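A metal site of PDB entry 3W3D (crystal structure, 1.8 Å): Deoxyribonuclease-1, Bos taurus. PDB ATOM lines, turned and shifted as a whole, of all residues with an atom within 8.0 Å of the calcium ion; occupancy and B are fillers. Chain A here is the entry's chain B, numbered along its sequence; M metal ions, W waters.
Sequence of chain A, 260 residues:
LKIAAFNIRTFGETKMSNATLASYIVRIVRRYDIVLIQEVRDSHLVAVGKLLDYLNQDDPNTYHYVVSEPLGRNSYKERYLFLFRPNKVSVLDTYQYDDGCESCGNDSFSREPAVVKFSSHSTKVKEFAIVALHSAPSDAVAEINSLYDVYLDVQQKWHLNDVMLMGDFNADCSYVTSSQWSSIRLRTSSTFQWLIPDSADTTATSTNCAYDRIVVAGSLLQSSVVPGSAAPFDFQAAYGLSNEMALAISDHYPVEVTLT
Of the 15 residues printed, 4 come within 4 Å of the calcium ion.
The nearest printed residue that does not touch the calcium ion is Ala 204 (4.2 Å).
The calcium ion is bound by O of Thr 205, water W1, O of Thr 207, O of Thr 203, OD2 of Asp 201, OD1 of Asp 201 and OG1 of Thr 203.
The calcium ion has seven donor atoms within binding distance.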
ATOM      1  N   ALA A 200      29.121  18.272 -13.680  1.00  0.00           N
ATOM      2  CA  ALA A 200      29.004  17.228 -12.690  1.00  0.00           C
ATOM      3  C   ALA A 200      27.709  17.415 -11.971  1.00  0.00           C
ATOM      4  O   ALA A 200      27.132  18.505 -11.856  1.00  0.00           O
ATOM      5  CB  ALA A 200      30.131  17.234 -11.597  1.00  0.00           C
ATOM      6  N   ASP A 201      27.354  16.290 -11.392  1.00  0.00           N
ATOM      7  CA  ASP A 201      26.205  16.271 -10.515  1.00  0.00           C
ATOM      8  C   ASP A 201      26.784  15.955  -9.154  1.00  0.00           C
ATOM      9  O   ASP A 201      27.239  14.806  -8.994  1.00  0.00           O
ATOM     10  CB  ASP A 201      25.254  15.168 -10.902  1.00  0.00           C
ATOM     11  CG  ASP A 201      23.994  15.111 -10.027  1.00  0.00           C
ATOM     12  OD1 ASP A 201      23.678  16.093  -9.352  1.00  0.00           O
ATOM     13  OD2 ASP A 201      23.319  14.077 -10.098  1.00  0.00           O
ATOM     14  N   THR A 202      26.787  16.867  -8.214  1.00  0.00           N
ATOM     15  CA  THR A 202      27.292  16.562  -6.874  1.00  0.00           C
ATOM     16  C   THR A 202      26.190  16.618  -5.816  1.00  0.00           C
ATOM     17  O   THR A 202      26.492  16.790  -4.644  1.00  0.00           O
ATOM     18  CB  THR A 202      28.362  17.553  -6.433  1.00  0.00           C
ATOM     19  OG1 THR A 202      27.835  18.872  -6.374  1.00  0.00           O
ATOM     20  CG2 THR A 202      29.454  17.572  -7.431  1.00  0.00           C
ATOM     21  N   THR A 203      24.912  16.600  -6.199  1.00  0.00           N
ATOM     22  CA  THR A 203      23.789  16.643  -5.276  1.00  0.00           C
ATOM     23  C   THR A 203      23.156  15.281  -5.188  1.00  0.00           C
ATOM     24  O   THR A 203      22.925  14.667  -6.228  1.00  0.00           O
ATOM     25  CB  THR A 203      22.725  17.598  -5.791  1.00  0.00           C
ATOM     26  OG1 THR A 203      22.373  17.137  -7.124  1.00  0.00           O
ATOM     27  CG2 THR A 203      23.221  19.023  -5.842  1.00  0.00           C
ATOM     28  N   ALA A 204      22.806  14.806  -4.013  1.00  0.00           N
ATOM     29  CA  ALA A 204      22.110  13.541  -3.877  1.00  0.00           C
ATOM     30  C   ALA A 204      20.688  13.683  -4.334  1.00  0.00           C
ATOM     31  O   ALA A 204      20.063  12.731  -4.777  1.00  0.00           O
ATOM     32  CB  ALA A 204      22.046  13.055  -2.433  1.00  0.00           C
ATOM     33  N   THR A 205      20.182  14.889  -4.311  1.00  0.00           N
ATOM     34  CA  THR A 205      18.837  15.169  -4.830  1.00  0.00           C
ATOM     35  C   THR A 205      18.719  15.020  -6.357  1.00  0.00           C
ATOM     36  O   THR A 205      19.723  14.929  -7.070  1.00  0.00           O
ATOM     37  CB  THR A 205      18.511  16.557  -4.398  1.00  0.00           C
ATOM     38  OG1 THR A 205      19.528  17.385  -4.969  1.00  0.00           O
ATOM     39  CG2 THR A 205      18.480  16.690  -2.886  1.00  0.00           C
ATOM     40  N   SER A 206      17.522  15.135  -6.885  1.00  0.00           N
ATOM     41  CA  SER A 206      17.169  14.997  -8.286  1.00  0.00           C
ATOM     42  C   SER A 206      17.594  16.166  -9.176  1.00  0.00           C
ATOM     43  O   SER A 206      17.357  16.229 -10.387  1.00  0.00           O
ATOM     44  CB  SER A 206      15.653  14.744  -8.313  1.00  0.00           C
ATOM     45  OG  SER A 206      14.964  15.356  -7.214  1.00  0.00           O
ATOM     46  N   THR A 207      18.258  17.111  -8.561  1.00  0.00           N
ATOM     47  CA  THR A 207      18.910  18.230  -9.165  1.00  0.00           C
ATOM     48  C   THR A 207      20.170  17.740  -9.786  1.00  0.00           C
ATOM     49  O   THR A 207      20.760  16.764  -9.262  1.00  0.00           O
ATOM     50  CB  THR A 207      19.071  19.173  -8.015  1.00  0.00           C
ATOM     51  OG1 THR A 207      18.049  20.143  -8.152  1.00  0.00           O
ATOM     52  CG2 THR A 207      20.389  19.815  -7.933  1.00  0.00           C
ATOM     53  N   ASN A 208      20.665  18.472 -10.808  1.00  0.00           N
ATOM     54  CA  ASN A 208      21.880  18.135 -11.529  1.00  0.00           C
ATOM     55  C   ASN A 208      22.726  19.390 -11.392  1.00  0.00           C
ATOM     56  O   ASN A 208      22.730  20.269 -12.236  1.00  0.00           O
ATOM     57  CB  ASN A 208      21.564  17.831 -12.997  1.00  0.00           C
ATOM     58  CG  ASN A 208      22.841  17.721 -13.804  1.00  0.00           C
ATOM     59  OD1 ASN A 208      23.751  17.115 -13.263  1.00  0.00           O
ATOM     60  ND2 ASN A 208      22.967  18.196 -15.056  1.00  0.00           N
ATOM     61  N   CYS A 209      23.437  19.554 -10.285  1.00  0.00           N
ATOM     62  CA  CYS A 209      24.169  20.788 -10.064  1.00  0.00           C
ATOM     63  C   CYS A 209      25.541  20.436  -9.546  1.00  0.00           C
ATOM     64  O   CYS A 209      25.597  19.494  -8.754  1.00  0.00           O
ATOM     65  CB  CYS A 209      23.404  21.646  -9.102  1.00  0.00           C
ATOM     66  SG  CYS A 209      21.678  21.983  -9.611  1.00  0.00           S
ATOM     67  N   ASP A 234      29.415   8.949  -5.717  1.00  0.00           N
ATOM     68  CA  ASP A 234      27.990   8.729  -5.483  1.00  0.00           C
ATOM     69  C   ASP A 234      27.845   7.484  -4.631  1.00  0.00           C
ATOM     70  O   ASP A 234      27.841   6.319  -5.075  1.00  0.00           O
ATOM     71  CB  ASP A 234      27.293   8.573  -6.825  1.00  0.00           C
ATOM     72  CG  ASP A 234      25.827   8.157  -6.822  1.00  0.00           C
ATOM     73  OD1 ASP A 234      25.302   8.067  -7.929  1.00  0.00           O
ATOM     74  OD2 ASP A 234      25.209   7.923  -5.777  1.00  0.00           O
ATOM     75  N   LEU A 247      19.316  10.165   0.879  1.00  0.00           N
ATOM     76  CA  LEU A 247      19.119  11.546   1.328  1.00  0.00           C
ATOM     77  C   LEU A 247      19.114  11.714   2.834  1.00  0.00           C
ATOM     78  O   LEU A 247      19.177  12.824   3.368  1.00  0.00           O
ATOM     79  CB  LEU A 247      17.809  12.109   0.815  1.00  0.00           C
ATOM     80  CG  LEU A 247      17.839  12.174  -0.698  1.00  0.00           C
ATOM     81  CD1 LEU A 247      16.426  12.384  -1.137  1.00  0.00           C
ATOM     82  CD2 LEU A 247      18.733  13.321  -1.240  1.00  0.00           C
ATOM     83  N   ASP A 251      22.065  15.514   1.286  1.00  0.00           N
ATOM     84  CA  ASP A 251      21.664  15.937  -0.044  1.00  0.00           C
ATOM     85  C   ASP A 251      22.875  16.280  -0.875  1.00  0.00           C
ATOM     86  O   ASP A 251      22.754  16.834  -1.989  1.00  0.00           O
ATOM     87  CB  ASP A 251      20.693  17.098   0.101  1.00  0.00           C
ATOM     88  CG  ASP A 251      21.045  18.324   0.867  1.00  0.00           C
ATOM     89  OD1 ASP A 251      22.186  18.484   1.303  1.00  0.00           O
ATOM     90  OD2 ASP A 251      20.135  19.117   0.965  1.00  0.00           O
ATOM     91  N   HIS A 252      24.114  15.989  -0.483  1.00  0.00           N
ATOM     92  CA  HIS A 252      25.229  16.251  -1.376  1.00  0.00           C
ATOM     93  C   HIS A 252      26.061  15.012  -1.465  1.00  0.00           C
ATOM     94  O   HIS A 252      25.916  14.117  -0.629  1.00  0.00           O
ATOM     95  CB  HIS A 252      26.107  17.293  -0.868  1.00  0.00           C
ATOM     96  CG  HIS A 252      25.592  18.706  -1.085  1.00  0.00           C
ATOM     97  ND1 HIS A 252      25.999  19.540  -2.012  1.00  0.00           N
ATOM     98  CD2 HIS A 252      24.675  19.361  -0.318  1.00  0.00           C
ATOM     99  CE1 HIS A 252      25.382  20.664  -1.811  1.00  0.00           C
ATOM    100  NE2 HIS A 252      24.581  20.565  -0.800  1.00  0.00           N
ATOM    101  N   TYR A 253      26.936  14.982  -2.482  1.00  0.00           N
ATOM    102  CA  TYR A 253      27.920  13.918  -2.636  1.00  0.00           C
ATOM    103  C   TYR A 253      29.241  14.500  -2.209  1.00  0.00           C
ATOM    104  O   TYR A 253      29.431  15.747  -2.392  1.00  0.00           O
ATOM    105  CB  TYR A 253      28.179  13.471  -4.066  1.00  0.00           C
ATOM    106  CG  TYR A 253      26.991  12.794  -4.671  1.00  0.00           C
ATOM    107  CD1 TYR A 253      26.734  13.010  -6.014  1.00  0.00           C
ATOM    108  CD2 TYR A 253      26.170  11.959  -3.897  1.00  0.00           C
ATOM    109  CE1 TYR A 253      25.626  12.397  -6.607  1.00  0.00           C
ATOM    110  CE2 TYR A 253      25.077  11.327  -4.496  1.00  0.00           C
ATOM    111  CZ  TYR A 253      24.819  11.557  -5.849  1.00  0.00           C
ATOM    112  OH  TYR A 253      23.688  10.984  -6.407  1.00  0.00           O
HETATM  113 CA    CA M   1      21.653  14.808  -8.265  1.00  0.00          CA
HETATM  114  O   HOH W   1      21.415  12.486  -8.061  1.00  0.00           O
